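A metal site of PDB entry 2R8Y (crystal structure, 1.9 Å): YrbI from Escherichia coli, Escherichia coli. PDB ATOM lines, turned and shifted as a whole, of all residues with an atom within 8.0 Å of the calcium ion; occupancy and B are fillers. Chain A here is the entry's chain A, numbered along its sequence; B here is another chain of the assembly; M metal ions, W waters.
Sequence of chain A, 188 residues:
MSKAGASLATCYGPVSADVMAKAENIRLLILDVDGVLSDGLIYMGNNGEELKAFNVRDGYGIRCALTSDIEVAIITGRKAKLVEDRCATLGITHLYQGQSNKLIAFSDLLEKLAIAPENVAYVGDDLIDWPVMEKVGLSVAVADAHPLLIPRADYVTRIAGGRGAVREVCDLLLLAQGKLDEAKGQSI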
ATOM      1  N   ASP A  32      28.710 -18.249   3.470  1.00  0.00           N
ATOM      2  CA  ASP A  32      27.313 -18.648   3.285  1.00  0.00           C
ATOM      3  C   ASP A  32      26.574 -18.555   4.642  1.00  0.00           C
ATOM      4  O   ASP A  32      27.208 -18.553   5.706  1.00  0.00           O
ATOM      5  CB  ASP A  32      27.249 -20.060   2.714  1.00  0.00           C
ATOM      6  CG  ASP A  32      25.835 -20.515   2.447  1.00  0.00           C
ATOM      7  OD1 ASP A  32      25.481 -21.626   2.893  1.00  0.00           O
ATOM      8  OD2 ASP A  32      25.064 -19.780   1.784  1.00  0.00           O
ATOM      9  N   VAL A  33      25.248 -18.474   4.600  1.00  0.00           N
ATOM     10  CA  VAL A  33      24.437 -18.467   5.820  1.00  0.00           C
ATOM     11  C   VAL A  33      23.932 -19.870   6.233  1.00  0.00           C
ATOM     12  O   VAL A  33      24.399 -20.449   7.212  1.00  0.00           O
ATOM     13  CB  VAL A  33      23.222 -17.504   5.691  1.00  0.00           C
ATOM     14  CG1 VAL A  33      22.402 -17.507   6.986  1.00  0.00           C
ATOM     15  CG2 VAL A  33      23.683 -16.090   5.400  1.00  0.00           C
ATOM     16  N   ASP A  34      22.999 -20.398   5.456  1.00  0.00           N
ATOM     17  CA  ASP A  34      22.276 -21.611   5.848  1.00  0.00           C
ATOM     18  C   ASP A  34      23.167 -22.860   5.772  1.00  0.00           C
ATOM     19  O   ASP A  34      23.560 -23.300   4.692  1.00  0.00           O
ATOM     20  CB  ASP A  34      21.013 -21.787   4.982  1.00  0.00           C
ATOM     21  CG  ASP A  34      20.012 -20.634   5.165  1.00  0.00           C
ATOM     22  OD1 ASP A  34      19.623 -20.351   6.314  1.00  0.00           O
ATOM     23  OD2 ASP A  34      19.628 -20.006   4.152  1.00  0.00           O
ATOM     24  N   GLY A  35      23.478 -23.440   6.924  1.00  0.00           N
ATOM     25  CA  GLY A  35      24.352 -24.635   6.928  1.00  0.00           C
ATOM     26  C   GLY A  35      25.801 -24.265   7.219  1.00  0.00           C
ATOM     27  O   GLY A  35      26.652 -25.145   7.366  1.00  0.00           O
ATOM     28  N   VAL A  36      26.093 -22.973   7.291  1.00  0.00           N
ATOM     29  CA  VAL A  36      27.438 -22.492   7.627  1.00  0.00           C
ATOM     30  C   VAL A  36      27.352 -21.644   8.891  1.00  0.00           C
ATOM     31  O   VAL A  36      27.943 -22.018   9.903  1.00  0.00           O
ATOM     32  CB  VAL A  36      28.133 -21.728   6.436  1.00  0.00           C
ATOM     33  CG1 VAL A  36      29.387 -20.946   6.911  1.00  0.00           C
ATOM     34  CG2 VAL A  36      28.492 -22.700   5.352  1.00  0.00           C
ATOM     35  N   LEU A  37      26.603 -20.542   8.829  1.00  0.00           N
ATOM     36  CA  LEU A  37      26.304 -19.726  10.021  1.00  0.00           C
ATOM     37  C   LEU A  37      25.170 -20.303  10.881  1.00  0.00           C
ATOM     38  O   LEU A  37      24.953 -19.859  12.006  1.00  0.00           O
ATOM     39  CB  LEU A  37      25.941 -18.297   9.622  1.00  0.00           C
ATOM     40  CG  LEU A  37      27.148 -17.424   9.267  1.00  0.00           C
ATOM     41  CD1 LEU A  37      26.699 -16.110   8.675  1.00  0.00           C
ATOM     42  CD2 LEU A  37      28.035 -17.176  10.505  1.00  0.00           C
ATOM     43  N   SER A  38      24.439 -21.265  10.309  1.00  0.00           N
ATOM     44  CA  SER A  38      23.339 -21.972  10.959  1.00  0.00           C
ATOM     45  C   SER A  38      23.556 -23.458  10.694  1.00  0.00           C
ATOM     46  O   SER A  38      24.439 -23.823   9.915  1.00  0.00           O
ATOM     47  CB  SER A  38      22.017 -21.543  10.355  1.00  0.00           C
ATOM     48  OG  SER A  38      21.865 -22.190   9.100  1.00  0.00           O
ATOM     49  N   GLY A  40      21.505 -25.197   9.060  1.00  0.00           N
ATOM     50  CA  GLY A  40      20.765 -25.470   7.827  1.00  0.00           C
ATOM     51  C   GLY A  40      19.256 -25.392   7.944  1.00  0.00           C
ATOM     52  O   GLY A  40      18.549 -25.553   6.941  1.00  0.00           O
ATOM     53  N   ILE A  75      27.130 -14.108   1.306  1.00  0.00           N
ATOM     54  CA  ILE A  75      26.360 -14.397   0.089  1.00  0.00           C
ATOM     55  C   ILE A  75      25.444 -15.593   0.339  1.00  0.00           C
ATOM     56  O   ILE A  75      25.909 -16.703   0.610  1.00  0.00           O
ATOM     57  CB  ILE A  75      27.273 -14.702  -1.111  1.00  0.00           C
ATOM     58  CG1 ILE A  75      28.298 -13.585  -1.347  1.00  0.00           C
ATOM     59  CG2 ILE A  75      26.411 -14.929  -2.384  1.00  0.00           C
ATOM     60  CD1 ILE A  75      29.444 -13.989  -2.275  1.00  0.00           C
ATOM     61  N   THR A  76      24.138 -15.357   0.209  1.00  0.00           N
ATOM     62  CA  THR A  76      23.127 -16.387   0.471  1.00  0.00           C
ATOM     63  C   THR A  76      22.050 -16.477  -0.622  1.00  0.00           C
ATOM     64  O   THR A  76      21.698 -15.481  -1.262  1.00  0.00           O
ATOM     65  CB  THR A  76      22.494 -16.206   1.902  1.00  0.00           C
ATOM     66  OG1 THR A  76      21.554 -17.241   2.153  1.00  0.00           O
ATOM     67  CG2 THR A  76      21.817 -14.836   2.072  1.00  0.00           C
ATOM     68  N   GLY A  77      21.548 -17.695  -0.850  1.00  0.00           N
ATOM     69  CA  GLY A  77      20.482 -17.931  -1.830  1.00  0.00           C
ATOM     70  C   GLY A  77      19.118 -17.476  -1.360  1.00  0.00           C
ATOM     71  O   GLY A  77      18.286 -17.120  -2.155  1.00  0.00           O
ATOM     72  N   LYS A 102      26.154 -17.260  -7.194  1.00  0.00           N
ATOM     73  CA  LYS A 102      26.995 -16.577  -6.206  1.00  0.00           C
ATOM     74  C   LYS A 102      28.204 -15.860  -6.822  1.00  0.00           C
ATOM     75  O   LYS A 102      28.829 -15.018  -6.182  1.00  0.00           O
ATOM     76  CB  LYS A 102      27.386 -17.518  -5.064  1.00  0.00           C
ATOM     77  CG  LYS A 102      26.192 -18.110  -4.339  1.00  0.00           C
ATOM     78  CD  LYS A 102      26.565 -18.539  -2.924  1.00  0.00           C
ATOM     79  CE  LYS A 102      25.337 -19.002  -2.181  1.00  0.00           C
ATOM     80  NZ  LYS A 102      25.641 -19.405  -0.762  1.00  0.00           N
ATOM     81  N   TYR A 122      36.459 -18.394   1.504  1.00  0.00           N
ATOM     82  CA  TYR A 122      35.022 -18.688   1.366  1.00  0.00           C
ATOM     83  C   TYR A 122      34.664 -19.954   2.141  1.00  0.00           C
ATOM     84  O   TYR A 122      35.311 -20.998   1.990  1.00  0.00           O
ATOM     85  CB  TYR A 122      34.609 -18.843  -0.106  1.00  0.00           C
ATOM     86  CG  TYR A 122      33.111 -18.900  -0.332  1.00  0.00           C
ATOM     87  CD1 TYR A 122      32.438 -17.843  -0.939  1.00  0.00           C
ATOM     88  CD2 TYR A 122      32.361 -20.022   0.057  1.00  0.00           C
ATOM     89  CE1 TYR A 122      31.049 -17.878  -1.139  1.00  0.00           C
ATOM     90  CE2 TYR A 122      30.981 -20.071  -0.138  1.00  0.00           C
ATOM     91  CZ  TYR A 122      30.333 -19.010  -0.741  1.00  0.00           C
ATOM     92  OH  TYR A 122      28.972 -19.061  -0.942  1.00  0.00           O
ATOM     93  N   VAL A 123      33.609 -19.852   2.931  1.00  0.00           N
ATOM     94  CA  VAL A 123      33.145 -20.972   3.727  1.00  0.00           C
ATOM     95  C   VAL A 123      31.758 -21.357   3.244  1.00  0.00           C
ATOM     96  O   VAL A 123      30.810 -20.582   3.378  1.00  0.00           O
ATOM     97  CB  VAL A 123      33.102 -20.642   5.245  1.00  0.00           C
ATOM     98  CG1 VAL A 123      32.862 -21.933   6.065  1.00  0.00           C
ATOM     99  CG2 VAL A 123      34.419 -19.979   5.716  1.00  0.00           C
ATOM    100  N   GLY A 124      31.664 -22.551   2.657  1.00  0.00           N
ATOM    101  CA  GLY A 124      30.406 -23.090   2.165  1.00  0.00           C
ATOM    102  C   GLY A 124      30.048 -24.465   2.712  1.00  0.00           C
ATOM    103  O   GLY A 124      30.827 -25.099   3.438  1.00  0.00           O
ATOM    104  N   ASP A 125      28.848 -24.924   2.349  1.00  0.00           N
ATOM    105  CA  ASP A 125      28.404 -26.250   2.773  1.00  0.00           C
ATOM    106  C   ASP A 125      27.692 -27.051   1.688  1.00  0.00           C
ATOM    107  O   ASP A 125      27.391 -28.211   1.905  1.00  0.00           O
ATOM    108  CB  ASP A 125      27.478 -26.123   4.000  1.00  0.00           C
ATOM    109  CG  ASP A 125      26.053 -25.804   3.593  1.00  0.00           C
ATOM    110  OD1 ASP A 125      25.111 -26.488   4.064  1.00  0.00           O
ATOM    111  OD2 ASP A 125      25.895 -24.893   2.749  1.00  0.00           O
ATOM    112  N   ASP A 126      27.402 -26.453   0.523  1.00  0.00           N
ATOM    113  CA  ASP A 126      26.699 -27.212  -0.523  1.00  0.00           C
ATOM    114  C   ASP A 126      27.249 -26.869  -1.917  1.00  0.00           C
ATOM    115  O   ASP A 126      28.079 -25.958  -2.079  1.00  0.00           O
ATOM    116  CB  ASP A 126      25.174 -26.984  -0.473  1.00  0.00           C
ATOM    117  CG  ASP A 126      24.359 -28.149  -1.025  1.00  0.00           C
ATOM    118  OD1 ASP A 126      24.921 -29.115  -1.602  1.00  0.00           O
ATOM    119  OD2 ASP A 126      23.110 -28.100  -0.915  1.00  0.00           O
ATOM    120  N   LEU A 127      26.772 -27.596  -2.915  1.00  0.00           N
ATOM    121  CA  LEU A 127      27.380 -27.556  -4.256  1.00  0.00           C
ATOM    122  C   LEU A 127      27.283 -26.180  -4.916  1.00  0.00           C
ATOM    123  O   LEU A 127      28.164 -25.796  -5.693  1.00  0.00           O
ATOM    124  CB  LEU A 127      26.801 -28.674  -5.122  1.00  0.00           C
ATOM    125  CG  LEU A 127      27.076 -30.118  -4.626  1.00  0.00           C
ATOM    126  CD1 LEU A 127      26.566 -31.149  -5.620  1.00  0.00           C
ATOM    127  CD2 LEU A 127      28.559 -30.403  -4.325  1.00  0.00           C
ATOM    128  N   ILE A 128      26.250 -25.422  -4.547  1.00  0.00           N
ATOM    129  CA  ILE A 128      26.035 -24.054  -5.046  1.00  0.00           C
ATOM    130  C   ILE A 128      27.163 -23.087  -4.631  1.00  0.00           C
ATOM    131  O   ILE A 128      27.388 -22.069  -5.285  1.00  0.00           O
ATOM    132  CB  ILE A 128      24.613 -23.553  -4.644  1.00  0.00           C
ATOM    133  CG1 ILE A 128      24.164 -22.373  -5.512  1.00  0.00           C
ATOM    134  CG2 ILE A 128      24.500 -23.312  -3.126  1.00  0.00           C
ATOM    135  CD1 ILE A 128      24.062 -22.700  -7.018  1.00  0.00           C
ATOM    136  N   ASP A 129      27.883 -23.438  -3.567  1.00  0.00           N
ATOM    137  CA  ASP A 129      29.031 -22.647  -3.124  1.00  0.00           C
ATOM    138  C   ASP A 129      30.302 -22.881  -3.933  1.00  0.00           C
ATOM    139  O   ASP A 129      31.226 -22.054  -3.896  1.00  0.00           O
ATOM    140  CB  ASP A 129      29.326 -22.951  -1.658  1.00  0.00           C
ATOM    141  CG  ASP A 129      28.186 -22.564  -0.767  1.00  0.00           C
ATOM    142  OD1 ASP A 129      27.806 -21.367  -0.798  1.00  0.00           O
ATOM    143  OD2 ASP A 129      27.625 -23.464  -0.095  1.00  0.00           O
ATOM    144  N   VAL A 142      32.465 -26.745   5.655  1.00  0.00           N
ATOM    145  CA  VAL A 142      32.173 -27.138   7.047  1.00  0.00           C
ATOM    146  C   VAL A 142      32.164 -28.660   7.213  1.00  0.00           C
ATOM    147  O   VAL A 142      31.983 -29.398   6.244  1.00  0.00           O
ATOM    148  CB  VAL A 142      30.870 -26.503   7.605  1.00  0.00           C
ATOM    149  CG1 VAL A 142      30.962 -24.972   7.587  1.00  0.00           C
ATOM    150  CG2 VAL A 142      29.653 -27.007   6.832  1.00  0.00           C
ATOM    151  N   ASN B  55      15.103 -28.142   6.181  1.00  0.00           N
ATOM    152  CA  ASN B  55      16.549 -28.090   5.931  1.00  0.00           C
ATOM    153  C   ASN B  55      16.788 -27.656   4.488  1.00  0.00           C
ATOM    154  O   ASN B  55      16.239 -28.250   3.552  1.00  0.00           O
ATOM    155  CB  ASN B  55      17.173 -29.463   6.181  1.00  0.00           C
ATOM    156  CG  ASN B  55      18.697 -29.405   6.357  1.00  0.00           C
ATOM    157  OD1 ASN B  55      19.227 -29.897   7.348  1.00  0.00           O
ATOM    158  ND2 ASN B  55      19.401 -28.835   5.396  1.00  0.00           N
ATOM    159  N   VAL B  56      17.609 -26.618   4.326  1.00  0.00           N
ATOM    160  CA  VAL B  56      17.910 -26.090   2.983  1.00  0.00           C
ATOM    161  C   VAL B  56      18.592 -27.112   2.059  1.00  0.00           C
ATOM    162  O   VAL B  56      18.488 -27.016   0.832  1.00  0.00           O
ATOM    163  CB  VAL B  56      18.773 -24.805   3.036  1.00  0.00           C
ATOM    164  CG1 VAL B  56      18.054 -23.708   3.807  1.00  0.00           C
ATOM    165  CG2 VAL B  56      20.170 -25.078   3.589  1.00  0.00           C
ATOM    166  N   ARG B  57      19.293 -28.060   2.661  1.00  0.00           N
ATOM    167  CA  ARG B  57      19.994 -29.081   1.892  1.00  0.00           C
ATOM    168  C   ARG B  57      18.975 -29.998   1.201  1.00  0.00           C
ATOM    169  O   ARG B  57      19.214 -30.447   0.079  1.00  0.00           O
ATOM    170  CB  ARG B  57      21.002 -29.832   2.759  1.00  0.00           C
ATOM    171  CG  ARG B  57      22.156 -28.897   3.202  1.00  0.00           C
ATOM    172  CD  ARG B  57      23.495 -29.269   2.576  1.00  0.00           C
ATOM    173  NE  ARG B  57      23.979 -30.490   3.190  1.00  0.00           N
ATOM    174  CZ  ARG B  57      24.855 -30.566   4.186  1.00  0.00           C
ATOM    175  NH1 ARG B  57      25.189 -31.777   4.633  1.00  0.00           N
ATOM    176  NH2 ARG B  57      25.415 -29.473   4.721  1.00  0.00           N
ATOM    177  N   SER B 187      19.869 -23.863  -2.785  1.00  0.00           N
ATOM    178  CA  SER B 187      19.902 -24.341  -1.401  1.00  0.00           C
ATOM    179  C   SER B 187      19.031 -23.404  -0.580  1.00  0.00           C
ATOM    180  O   SER B 187      19.539 -22.463   0.074  1.00  0.00           O
ATOM    181  CB  SER B 187      21.340 -24.401  -0.874  1.00  0.00           C
ATOM    182  OG  SER B 187      21.535 -25.496   0.023  1.00  0.00           O
ATOM    183  N   ILE B 188      17.713 -23.620  -0.660  1.00  0.00           N
ATOM    184  CA  ILE B 188      16.733 -22.721  -0.019  1.00  0.00           C
ATOM    185  C   ILE B 188      15.700 -23.458   0.850  1.00  0.00           C
ATOM    186  O   ILE B 188      14.942 -22.827   1.600  1.00  0.00           O
ATOM    187  CB  ILE B 188      15.982 -21.855  -1.073  1.00  0.00           C
ATOM    188  CG1 ILE B 188      15.209 -22.751  -2.066  1.00  0.00           C
ATOM    189  CG2 ILE B 188      16.950 -20.883  -1.752  1.00  0.00           C
ATOM    190  CD1 ILE B 188      14.421 -22.015  -3.161  1.00  0.00           C
ATOM    191  OXT ILE B 188      15.582 -24.683   0.817  1.00  0.00           O
HETATM  192 CA    CA M   1      24.264 -23.435   2.482  1.00  0.00          CA
HETATM  193  O   HOH W   1      25.003 -23.160   0.186  1.00  0.00           O
HETATM  194  O   HOH W   2      23.107 -25.550   2.261  1.00  0.00           O
HETATM  195  O   HOH W   3      22.342 -22.427   1.493  1.00  0.00           O
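The calcium ion is bound by OD2 of Asp 125 (2.2 Å), OD1 of Asp 32 (2.2 Å), O of Asp 34 (2.3 Å), water W3 (2.4 Å), water W2 (2.4 Å) and water W1 (2.4 Å).
The calcium ion has six donor atoms within binding distance.
Water W2 lies within hydrogen-bond range of OG of Ser 187 of chain B (2.7 Å) and OD1 of Asp 125 (2.9 Å).
OD2 of Asp 129 sits at hydrogen-bond distance from N of Asp 125.
The side-chain carboxylate of Asp 125 lies within salt-bridge range of the guanidinium group of Arg 57 of chain B (3.1 Å).
OD2 of Asp 32 lies within salt-bridge range of NZ of Lys 102.
The backbone NH (N) of Asp 32 sits at hydrogen-bond distance from the backbone carbonyl oxygen (O) of Val 123, at 3.1 Å.
Of the 26 residues printed, 3 come within 4 Å of the calcium ion.
Along chain A the residues within 4 Å of the calcium ion span positions 32 to 125.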
